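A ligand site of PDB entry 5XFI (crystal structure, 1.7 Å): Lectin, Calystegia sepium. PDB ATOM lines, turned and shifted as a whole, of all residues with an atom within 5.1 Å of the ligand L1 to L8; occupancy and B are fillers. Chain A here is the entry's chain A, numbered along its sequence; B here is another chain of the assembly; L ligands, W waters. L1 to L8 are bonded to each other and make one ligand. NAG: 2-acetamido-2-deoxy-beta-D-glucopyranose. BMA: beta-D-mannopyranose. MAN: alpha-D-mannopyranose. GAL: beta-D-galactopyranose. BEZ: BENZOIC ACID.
An oxygen (O6) of MAN L5 is in hydrogen-bond range of an oxygen (O2) of BEZ L9 (2.8 Å).
CA of Gly 16 touches O4 of MAN L4, 3.6 Å away.
O of Gly 64 touches C8 of NAG L6, at 3.4 Å.
O of Leu 94 touches C5 of NAG L2 (3.4 Å).
O of Val 25 of chain B touches O6 of GAL L8, 3.9 Å away.
Arg 151 of chain B touches the ligand L1 to L8.
Hydrophobic or aromatic side chains that line the ligand L1 to L8: Leu 94, Tyr 141 and Tyr 142.
OD1 of Asp 144 lies within hydrogen-bond range of N of Gly 140.
The backbone NH of Asn 18 sits at hydrogen-bond distance from the backbone carbonyl oxygen of Ser 139 (2.7 Å).
N of Gly 64 sits at hydrogen-bond distance from O of Gly 140 (3.0 Å).
The side-chain amide oxygen of Asn 96 sits close to the backbone carbonyl oxygen of Leu 94, 2.9 Å away.
The side-chain carboxylate of Asp 67 is in hydrogen-bond range of the side-chain hydroxyl of Tyr 142 (2.7 Å).
The side-chain amide nitrogen (ND2) of Asn 18 is in hydrogen-bond range of an oxygen (O3) of NAG L6, at 3.0 Å.
N of Tyr 141 sits at hydrogen-bond distance from O6 of MAN L4, at 3.0 Å.
The side-chain carboxylate (OD2) of Asp 144 is in hydrogen-bond range of an oxygen (O4) of MAN L4 (2.6 Å).
The backbone NH of Gly 140 is in hydrogen-bond range of an oxygen (O6) of MAN L4, at 3.1 Å.
The backbone NH (N) of Gly 17 lies within hydrogen-bond range of an oxygen (O3) of MAN L4, at 2.9 Å.
The backbone carbonyl oxygen of Tyr 142 sits at hydrogen-bond distance from an oxygen (O6) of MAN L4 (3.3 Å).
N of Tyr 142 lies within hydrogen-bond range of O6 of MAN L4, 2.9 Å away.
OD2 of Asp 95 lies within hydrogen-bond range of N2 of NAG L2, 2.9 Å away.
ND2 of Asn 96 lies within hydrogen-bond range of O2 of BMA L3 (2.6 Å).
Water W4 bridges an oxygen (O3) of NAG L1 and the side-chain carboxylate (OD2) of Asp 67.
Water W3 bridges an oxygen (O6) of NAG L2 (2.7 Å) and the side-chain carboxylate (OD1) of Asp 67 (2.7 Å).
Water W1 lies within hydrogen-bond range of the backbone carbonyl oxygen of Val 25 of chain B (2.5 Å), an oxygen (O6) of GAL L8 (2.7 Å), the guanidinium group of Arg 151 of chain B (2.9 Å) and the side-chain amide oxygen of Asn 18 (3.3 Å).
Water W7 bridges the side-chain amide nitrogen of Asn 96 (2.7 Å) and an oxygen (O4) of MAN L4 (3.1 Å).
Water W5 bridges O of Gly 17 (2.7 Å) and O6 of NAG L6 (3.2 Å).
Water W2 bridges the side-chain carboxylate of Asp 144 and an oxygen (O4) of MAN L4.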
ATOM      1  N   GLY A  16     -25.923  28.705  -7.717  1.00  0.00           N
ATOM      2  CA  GLY A  16     -26.786  28.483  -8.855  1.00  0.00           C
ATOM      3  C   GLY A  16     -26.529  27.160  -9.536  1.00  0.00           C
ATOM      4  O   GLY A  16     -25.654  26.368  -9.148  1.00  0.00           O
ATOM      5  N   GLY A  17     -27.365  26.867 -10.545  1.00  0.00           N
ATOM      6  CA  GLY A  17     -27.142  25.699 -11.369  1.00  0.00           C
ATOM      7  C   GLY A  17     -27.432  24.400 -10.659  1.00  0.00           C
ATOM      8  O   GLY A  17     -28.166  24.340  -9.653  1.00  0.00           O
ATOM      9  N   ASN A  18     -26.832  23.337 -11.203  1.00  0.00           N
ATOM     10  CA  ASN A  18     -26.974  21.968 -10.762  1.00  0.00           C
ATOM     11  C   ASN A  18     -25.660  21.484 -10.182  1.00  0.00           C
ATOM     12  O   ASN A  18     -24.599  21.790 -10.720  1.00  0.00           O
ATOM     13  CB  ASN A  18     -27.324  21.033 -11.939  1.00  0.00           C
ATOM     14  CG  ASN A  18     -28.575  21.435 -12.647  1.00  0.00           C
ATOM     15  OD1 ASN A  18     -29.647  21.384 -12.048  1.00  0.00           O
ATOM     16  ND2 ASN A  18     -28.454  21.888 -13.910  1.00  0.00           N
ATOM     17  N   GLY A  64     -24.970  24.463 -20.652  1.00  0.00           N
ATOM     18  CA  GLY A  64     -26.318  23.907 -20.657  1.00  0.00           C
ATOM     19  C   GLY A  64     -27.346  24.737 -21.397  1.00  0.00           C
ATOM     20  O   GLY A  64     -28.440  24.239 -21.685  1.00  0.00           O
ATOM     21  N   GLY A  65     -27.024  26.010 -21.688  1.00  0.00           N
ATOM     22  CA  GLY A  65     -27.916  26.877 -22.425  1.00  0.00           C
ATOM     23  C   GLY A  65     -27.626  26.829 -23.914  1.00  0.00           C
ATOM     24  O   GLY A  65     -26.940  25.926 -24.409  1.00  0.00           O
ATOM     25  N   ASP A  67     -25.839  28.829 -25.775  1.00  0.00           N
ATOM     26  CA  ASP A  67     -24.640  29.550 -26.205  1.00  0.00           C
ATOM     27  C   ASP A  67     -23.824  28.737 -27.178  1.00  0.00           C
ATOM     28  O   ASP A  67     -23.551  27.550 -26.947  1.00  0.00           O
ATOM     29  CB  ASP A  67     -23.743  29.862 -25.005  1.00  0.00           C
ATOM     30  CG  ASP A  67     -24.468  30.594 -23.893  1.00  0.00           C
ATOM     31  OD1 ASP A  67     -25.419  30.026 -23.324  1.00  0.00           O
ATOM     32  OD2 ASP A  67     -24.059  31.731 -23.587  1.00  0.00           O
ATOM     33  N   LEU A  94     -22.625  37.852 -18.861  1.00  0.00           N
ATOM     34  CA  LEU A  94     -24.019  37.938 -19.321  1.00  0.00           C
ATOM     35  C   LEU A  94     -25.012  37.845 -18.149  1.00  0.00           C
ATOM     36  O   LEU A  94     -25.962  37.043 -18.165  1.00  0.00           O
ATOM     37  CB  LEU A  94     -24.318  36.870 -20.373  1.00  0.00           C
ATOM     38  CG  LEU A  94     -23.417  36.875 -21.613  1.00  0.00           C
ATOM     39  CD1 LEU A  94     -23.901  35.777 -22.558  1.00  0.00           C
ATOM     40  CD2 LEU A  94     -23.425  38.247 -22.311  1.00  0.00           C
ATOM     41  N   ASP A  95     -24.774  38.671 -17.131  1.00  0.00           N
ATOM     42  CA  ASP A  95     -25.643  38.807 -15.959  1.00  0.00           C
ATOM     43  C   ASP A  95     -25.650  37.566 -15.076  1.00  0.00           C
ATOM     44  O   ASP A  95     -26.634  37.301 -14.365  1.00  0.00           O
ATOM     45  CB  ASP A  95     -27.085  39.149 -16.348  1.00  0.00           C
ATOM     46  CG  ASP A  95     -27.190  40.437 -17.129  1.00  0.00           C
ATOM     47  OD1 ASP A  95     -26.633  41.458 -16.692  1.00  0.00           O
ATOM     48  OD2 ASP A  95     -27.834  40.428 -18.197  1.00  0.00           O
ATOM     49  N   ASN A  96     -24.581  36.772 -15.123  1.00  0.00           N
ATOM     50  CA  ASN A  96     -24.437  35.613 -14.260  1.00  0.00           C
ATOM     51  C   ASN A  96     -23.089  35.660 -13.559  1.00  0.00           C
ATOM     52  O   ASN A  96     -22.080  35.962 -14.182  1.00  0.00           O
ATOM     53  CB  ASN A  96     -24.499  34.325 -15.068  1.00  0.00           C
ATOM     54  CG  ASN A  96     -25.890  34.063 -15.602  1.00  0.00           C
ATOM     55  OD1 ASN A  96     -26.256  34.549 -16.686  1.00  0.00           O
ATOM     56  ND2 ASN A  96     -26.659  33.288 -14.855  1.00  0.00           N
ATOM     57  N   VAL A  98     -20.291  33.748 -12.443  1.00  0.00           N
ATOM     58  CA  VAL A  98     -19.860  32.420 -12.850  1.00  0.00           C
ATOM     59  C   VAL A  98     -18.343  32.434 -13.032  1.00  0.00           C
ATOM     60  O   VAL A  98     -17.686  33.464 -12.873  1.00  0.00           O
ATOM     61  CB  VAL A  98     -20.568  31.956 -14.141  1.00  0.00           C
ATOM     62  CG1 VAL A  98     -22.091  31.788 -13.914  1.00  0.00           C
ATOM     63  CG2 VAL A  98     -20.301  32.916 -15.281  1.00  0.00           C
ATOM     64  N   SER A 139     -23.211  23.824 -12.005  1.00  0.00           N
ATOM     65  CA  SER A 139     -23.185  24.368 -13.365  1.00  0.00           C
ATOM     66  C   SER A 139     -24.609  24.410 -13.920  1.00  0.00           C
ATOM     67  O   SER A 139     -25.476  23.631 -13.510  1.00  0.00           O
ATOM     68  CB  SER A 139     -22.277  23.539 -14.297  1.00  0.00           C
ATOM     69  OG  SER A 139     -22.826  22.234 -14.458  1.00  0.00           O
ATOM     70  N   GLY A 140     -24.802  25.340 -14.855  1.00  0.00           N
ATOM     71  CA  GLY A 140     -26.053  25.461 -15.588  1.00  0.00           C
ATOM     72  C   GLY A 140     -25.735  25.866 -17.018  1.00  0.00           C
ATOM     73  O   GLY A 140     -25.152  25.075 -17.770  1.00  0.00           O
ATOM     74  N   TYR A 141     -26.072  27.101 -17.391  1.00  0.00           N
ATOM     75  CA  TYR A 141     -25.530  27.637 -18.642  1.00  0.00           C
ATOM     76  C   TYR A 141     -24.022  27.694 -18.587  1.00  0.00           C
ATOM     77  O   TYR A 141     -23.339  27.514 -19.605  1.00  0.00           O
ATOM     78  CB  TYR A 141     -26.072  29.045 -18.902  1.00  0.00           C
ATOM     79  CG  TYR A 141     -27.481  29.139 -19.424  1.00  0.00           C
ATOM     80  CD1 TYR A 141     -28.441  28.155 -19.140  1.00  0.00           C
ATOM     81  CD2 TYR A 141     -27.842  30.212 -20.227  1.00  0.00           C
ATOM     82  CE1 TYR A 141     -29.725  28.251 -19.614  1.00  0.00           C
ATOM     83  CE2 TYR A 141     -29.155  30.327 -20.731  1.00  0.00           C
ATOM     84  CZ  TYR A 141     -30.083  29.343 -20.408  1.00  0.00           C
ATOM     85  OH  TYR A 141     -31.370  29.486 -20.894  1.00  0.00           O
ATOM     86  N   TYR A 142     -23.480  28.021 -17.402  1.00  0.00           N
ATOM     87  CA  TYR A 142     -22.059  28.296 -17.241  1.00  0.00           C
ATOM     88  C   TYR A 142     -21.563  27.515 -16.029  1.00  0.00           C
ATOM     89  O   TYR A 142     -22.267  26.629 -15.540  1.00  0.00           O
ATOM     90  CB  TYR A 142     -21.828  29.810 -17.058  1.00  0.00           C
ATOM     91  CG  TYR A 142     -22.522  30.605 -18.117  1.00  0.00           C
ATOM     92  CD1 TYR A 142     -22.307  30.323 -19.461  1.00  0.00           C
ATOM     93  CD2 TYR A 142     -23.449  31.587 -17.789  1.00  0.00           C
ATOM     94  CE1 TYR A 142     -22.973  31.025 -20.465  1.00  0.00           C
ATOM     95  CE2 TYR A 142     -24.111  32.299 -18.773  1.00  0.00           C
ATOM     96  CZ  TYR A 142     -23.866  32.004 -20.111  1.00  0.00           C
ATOM     97  OH  TYR A 142     -24.530  32.693 -21.118  1.00  0.00           O
ATOM     98  N   VAL A 143     -20.372  27.814 -15.522  1.00  0.00           N
ATOM     99  CA  VAL A 143     -19.843  27.097 -14.366  1.00  0.00           C
ATOM    100  C   VAL A 143     -20.077  27.955 -13.130  1.00  0.00           C
ATOM    101  O   VAL A 143     -19.465  29.026 -12.978  1.00  0.00           O
ATOM    102  CB  VAL A 143     -18.360  26.743 -14.541  1.00  0.00           C
ATOM    103  CG1 VAL A 143     -17.837  26.050 -13.260  1.00  0.00           C
ATOM    104  CG2 VAL A 143     -18.187  25.841 -15.750  1.00  0.00           C
ATOM    105  N   ASP A 144     -20.974  27.507 -12.256  1.00  0.00           N
ATOM    106  CA  ASP A 144     -21.343  28.307 -11.084  1.00  0.00           C
ATOM    107  C   ASP A 144     -20.421  28.121  -9.890  1.00  0.00           C
ATOM    108  O   ASP A 144     -20.301  29.041  -9.067  1.00  0.00           O
ATOM    109  CB  ASP A 144     -22.761  27.973 -10.645  1.00  0.00           C
ATOM    110  CG  ASP A 144     -23.764  28.297 -11.705  1.00  0.00           C
ATOM    111  OD1 ASP A 144     -24.025  27.418 -12.573  1.00  0.00           O
ATOM    112  OD2 ASP A 144     -24.272  29.445 -11.685  1.00  0.00           O
ATOM    113  N   VAL B  25     -24.620  16.339 -15.222  1.00  0.00           N
ATOM    114  CA  VAL B  25     -25.678  17.339 -15.115  1.00  0.00           C
ATOM    115  C   VAL B  25     -26.997  16.870 -15.723  1.00  0.00           C
ATOM    116  O   VAL B  25     -28.071  17.218 -15.231  1.00  0.00           O
ATOM    117  CB  VAL B  25     -25.209  18.658 -15.740  1.00  0.00           C
ATOM    118  CG1 VAL B  25     -26.370  19.630 -15.862  1.00  0.00           C
ATOM    119  CG2 VAL B  25     -24.109  19.261 -14.855  1.00  0.00           C
ATOM    120  N   ARG B 151     -31.747  14.084  -5.495  1.00  0.00           N
ATOM    121  CA  ARG B 151     -32.376  15.373  -5.763  1.00  0.00           C
ATOM    122  C   ARG B 151     -33.881  15.155  -5.902  1.00  0.00           C
ATOM    123  O   ARG B 151     -34.337  14.210  -6.539  1.00  0.00           O
ATOM    124  CB  ARG B 151     -31.815  16.038  -7.044  1.00  0.00           C
ATOM    125  CG  ARG B 151     -32.532  17.333  -7.475  1.00  0.00           C
ATOM    126  CD  ARG B 151     -32.211  17.728  -8.946  1.00  0.00           C
ATOM    127  NE  ARG B 151     -32.772  16.796  -9.932  1.00  0.00           N
ATOM    128  CZ  ARG B 151     -32.283  16.610 -11.164  1.00  0.00           C
ATOM    129  NH1 ARG B 151     -31.195  17.268 -11.574  1.00  0.00           N
ATOM    130  NH2 ARG B 151     -32.855  15.734 -11.989  1.00  0.00           N
ATOM    131  N   HIS B 152     -34.649  16.039  -5.294  1.00  0.00           N
ATOM    132  CA  HIS B 152     -36.081  15.800  -5.275  1.00  0.00           C
ATOM    133  C   HIS B 152     -36.737  16.393  -6.514  1.00  0.00           C
ATOM    134  O   HIS B 152     -36.299  17.429  -7.043  1.00  0.00           O
ATOM    135  CB  HIS B 152     -36.720  16.372  -4.006  1.00  0.00           C
ATOM    136  CG  HIS B 152     -37.802  15.502  -3.470  1.00  0.00           C
ATOM    137  ND1 HIS B 152     -39.128  15.651  -3.837  1.00  0.00           N
ATOM    138  CD2 HIS B 152     -37.757  14.437  -2.640  1.00  0.00           C
ATOM    139  CE1 HIS B 152     -39.847  14.719  -3.243  1.00  0.00           C
ATOM    140  NE2 HIS B 152     -39.041  13.968  -2.507  1.00  0.00           N
HETATM  141  C1  NAG L   1     -27.141  39.136 -25.989  1.00  0.00           C
HETATM  142  C2  NAG L   1     -26.946  37.684 -25.613  1.00  0.00           C
HETATM  143  C3  NAG L   1     -27.828  37.329 -24.409  1.00  0.00           C
HETATM  144  C4  NAG L   1     -27.626  38.305 -23.256  1.00  0.00           C
HETATM  145  C5  NAG L   1     -27.561  39.766 -23.712  1.00  0.00           C
HETATM  146  C6  NAG L   1     -26.893  40.651 -22.697  1.00  0.00           C
HETATM  147  C7  NAG L   1     -26.297  36.272 -27.514  1.00  0.00           C
HETATM  148  C8  NAG L   1     -26.778  35.383 -28.620  1.00  0.00           C
HETATM  149  N2  NAG L   1     -27.240  36.800 -26.739  1.00  0.00           N
HETATM  150  O1  NAG L   1     -26.306  39.455 -27.057  1.00  0.00           O
HETATM  151  O3  NAG L   1     -27.491  36.010 -24.001  1.00  0.00           O
HETATM  152  O4  NAG L   1     -28.721  38.191 -22.337  1.00  0.00           O
HETATM  153  O5  NAG L   1     -26.788  39.931 -24.916  1.00  0.00           O
HETATM  154  O6  NAG L   1     -27.565  40.627 -21.453  1.00  0.00           O
HETATM  155  O7  NAG L   1     -25.098  36.486 -27.329  1.00  0.00           O
HETATM  156  C1  NAG L   2     -28.458  37.449 -21.098  1.00  0.00           C
HETATM  157  C2  NAG L   2     -29.661  37.593 -20.142  1.00  0.00           C
HETATM  158  C3  NAG L   2     -29.470  36.704 -18.911  1.00  0.00           C
HETATM  159  C4  NAG L   2     -29.163  35.277 -19.334  1.00  0.00           C
HETATM  160  C5  NAG L   2     -27.949  35.293 -20.247  1.00  0.00           C
HETATM  161  C6  NAG L   2     -27.575  33.918 -20.772  1.00  0.00           C
HETATM  162  C7  NAG L   2     -30.767  39.778 -20.245  1.00  0.00           C
HETATM  163  C8  NAG L   2     -30.800  41.177 -19.715  1.00  0.00           C
HETATM  164  N2  NAG L   2     -29.824  38.975 -19.738  1.00  0.00           N
HETATM  165  O3  NAG L   2     -30.653  36.746 -18.111  1.00  0.00           O
HETATM  166  O4  NAG L   2     -28.868  34.510 -18.174  1.00  0.00           O
HETATM  167  O5  NAG L   2     -28.242  36.094 -21.394  1.00  0.00           O
HETATM  168  O6  NAG L   2     -28.608  33.439 -21.622  1.00  0.00           O
HETATM  169  O7  NAG L   2     -31.552  39.389 -21.100  1.00  0.00           O
HETATM  170  C1  BMA L   3     -29.616  33.270 -18.151  1.00  0.00           C
HETATM  171  C2  BMA L   3     -29.072  32.437 -16.972  1.00  0.00           C
HETATM  172  C3  BMA L   3     -29.825  31.143 -16.812  1.00  0.00           C
HETATM  173  C4  BMA L   3     -31.363  31.390 -16.777  1.00  0.00           C
HETATM  174  C5  BMA L   3     -31.800  32.315 -17.953  1.00  0.00           C
HETATM  175  C6  BMA L   3     -33.266  32.765 -17.823  1.00  0.00           C
HETATM  176  O2  BMA L   3     -29.166  33.197 -15.699  1.00  0.00           O
HETATM  177  O3  BMA L   3     -29.493  30.549 -15.596  1.00  0.00           O
HETATM  178  O4  BMA L   3     -32.032  30.167 -16.911  1.00  0.00           O
HETATM  179  O5  BMA L   3     -30.983  33.505 -17.979  1.00  0.00           O
HETATM  180  O6  BMA L   3     -33.472  33.278 -16.506  1.00  0.00           O
HETATM  181  C1  MAN L   4     -29.014  29.207 -15.673  1.00  0.00           C
HETATM  182  C2  MAN L   4     -29.545  28.535 -14.409  1.00  0.00           C
HETATM  183  C3  MAN L   4     -28.894  29.129 -13.156  1.00  0.00           C
HETATM  184  C4  MAN L   4     -27.326  29.171 -13.259  1.00  0.00           C
HETATM  185  C5  MAN L   4     -26.940  29.817 -14.596  1.00  0.00           C
HETATM  186  C6  MAN L   4     -25.452  29.825 -14.845  1.00  0.00           C
HETATM  187  O2  MAN L   4     -29.223  27.138 -14.488  1.00  0.00           O
HETATM  188  O3  MAN L   4     -29.292  28.459 -11.946  1.00  0.00           O
HETATM  189  O4  MAN L   4     -26.738  29.930 -12.169  1.00  0.00           O
HETATM  190  O5  MAN L   4     -27.596  29.116 -15.706  1.00  0.00           O
HETATM  191  O6  MAN L   4     -24.955  28.481 -14.935  1.00  0.00           O
HETATM  192  C1  MAN L   5     -33.524  34.727 -16.524  1.00  0.00           C
HETATM  193  C2  MAN L   5     -33.644  35.210 -15.068  1.00  0.00           C
HETATM  194  C3  MAN L   5     -34.938  34.662 -14.528  1.00  0.00           C
HETATM  195  C4  MAN L   5     -36.109  35.221 -15.340  1.00  0.00           C
HETATM  196  C5  MAN L   5     -35.956  34.916 -16.837  1.00  0.00           C
HETATM  197  C6  MAN L   5     -36.904  35.721 -17.696  1.00  0.00           C
HETATM  198  O2  MAN L   5     -33.816  36.636 -15.004  1.00  0.00           O
HETATM  199  O3  MAN L   5     -35.095  34.978 -13.151  1.00  0.00           O
HETATM  200  O4  MAN L   5     -37.290  34.602 -14.897  1.00  0.00           O
HETATM  201  O5  MAN L   5     -34.610  35.230 -17.314  1.00  0.00           O
HETATM  202  O6  MAN L   5     -36.452  35.641 -19.052  1.00  0.00           O
HETATM  203  C1  NAG L   6     -30.360  26.355 -14.124  1.00  0.00           C
HETATM  204  C2  NAG L   6     -30.238  24.985 -14.799  1.00  0.00           C
HETATM  205  C3  NAG L   6     -31.408  24.095 -14.382  1.00  0.00           C
HETATM  206  C4  NAG L   6     -31.595  24.088 -12.870  1.00  0.00           C
HETATM  207  C5  NAG L   6     -31.546  25.486 -12.274  1.00  0.00           C
HETATM  208  C6  NAG L   6     -31.493  25.466 -10.772  1.00  0.00           C
HETATM  209  C7  NAG L   6     -29.352  24.444 -17.039  1.00  0.00           C
HETATM  210  C8  NAG L   6     -29.461  24.723 -18.515  1.00  0.00           C
HETATM  211  N2  NAG L   6     -30.201  25.127 -16.249  1.00  0.00           N
HETATM  212  O3  NAG L   6     -31.154  22.781 -14.861  1.00  0.00           O
HETATM  213  O4  NAG L   6     -32.902  23.614 -12.569  1.00  0.00           O
HETATM  214  O5  NAG L   6     -30.389  26.187 -12.732  1.00  0.00           O
HETATM  215  O6  NAG L   6     -31.449  26.784 -10.237  1.00  0.00           O
HETATM  216  O7  NAG L   6     -28.539  23.644 -16.596  1.00  0.00           O
HETATM  217  C1  NAG L   7     -32.569  37.313 -14.819  1.00  0.00           C
HETATM  218  C2  NAG L   7     -32.550  38.551 -15.708  1.00  0.00           C
HETATM  219  C3  NAG L   7     -31.277  39.356 -15.494  1.00  0.00           C
HETATM  220  C4  NAG L   7     -31.055  39.652 -14.017  1.00  0.00           C
HETATM  221  C5  NAG L   7     -31.122  38.363 -13.201  1.00  0.00           C
HETATM  222  C6  NAG L   7     -31.024  38.610 -11.709  1.00  0.00           C
HETATM  223  C7  NAG L   7     -33.841  38.207 -17.793  1.00  0.00           C
HETATM  224  C8  NAG L   7     -33.769  37.785 -19.225  1.00  0.00           C
HETATM  225  N2  NAG L   7     -32.682  38.179 -17.113  1.00  0.00           N
HETATM  226  O3  NAG L   7     -31.359  40.569 -16.232  1.00  0.00           O
HETATM  227  O4  NAG L   7     -29.771  40.242 -13.822  1.00  0.00           O
HETATM  228  O5  NAG L   7     -32.372  37.692 -13.439  1.00  0.00           O
HETATM  229  O6  NAG L   7     -31.190  37.421 -10.949  1.00  0.00           O
HETATM  230  O7  NAG L   7     -34.896  38.560 -17.256  1.00  0.00           O
HETATM  231  C1  GAL L   8     -32.853  22.237 -12.203  1.00  0.00           C
HETATM  232  C2  GAL L   8     -34.144  21.945 -11.471  1.00  0.00           C
HETATM  233  C3  GAL L   8     -34.270  20.474 -11.134  1.00  0.00           C
HETATM  234  C4  GAL L   8     -34.092  19.616 -12.391  1.00  0.00           C
HETATM  235  C5  GAL L   8     -32.780  20.049 -13.039  1.00  0.00           C
HETATM  236  C6  GAL L   8     -32.429  19.354 -14.334  1.00  0.00           C
HETATM  237  O2  GAL L   8     -34.210  22.649 -10.276  1.00  0.00           O
HETATM  238  O3  GAL L   8     -35.594  20.241 -10.595  1.00  0.00           O
HETATM  239  O4  GAL L   8     -35.149  19.856 -13.310  1.00  0.00           O
HETATM  240  O5  GAL L   8     -32.795  21.449 -13.342  1.00  0.00           O
HETATM  241  O6  GAL L   8     -31.073  19.671 -14.708  1.00  0.00           O
HETATM  242  C   BEZ L   9     -35.286  32.430 -20.527  1.00  0.00           C
HETATM  243  O1  BEZ L   9     -35.291  31.186 -20.652  1.00  0.00           O
HETATM  244  O2  BEZ L   9     -36.266  32.997 -19.955  1.00  0.00           O
HETATM  245  C1  BEZ L   9     -34.138  33.256 -21.039  1.00  0.00           C
HETATM  246  C2  BEZ L   9     -32.866  32.668 -21.206  1.00  0.00           C
HETATM  247  C3  BEZ L   9     -31.779  33.430 -21.671  1.00  0.00           C
HETATM  248  C4  BEZ L   9     -32.000  34.790 -21.969  1.00  0.00           C
HETATM  249  C5  BEZ L   9     -33.264  35.368 -21.814  1.00  0.00           C
HETATM  250  C6  BEZ L   9     -34.334  34.608 -21.347  1.00  0.00           C
HETATM  251  O   HOH W   1     -29.156  18.377 -13.242  1.00  0.00           O
HETATM  252  O   HOH W   2     -24.241  31.846 -10.724  1.00  0.00           O
HETATM  253  O   HOH W   3     -27.443  31.852 -23.505  1.00  0.00           O
HETATM  254  O   HOH W   4     -26.338  33.833 -25.081  1.00  0.00           O
HETATM  255  O   HOH W   5     -29.372  26.119  -7.946  1.00  0.00           O
HETATM  256  O   HOH W   6     -23.945  34.108 -26.320  1.00  0.00           O
HETATM  257  O   HOH W   7     -26.655  32.983 -12.183  1.00  0.00           O
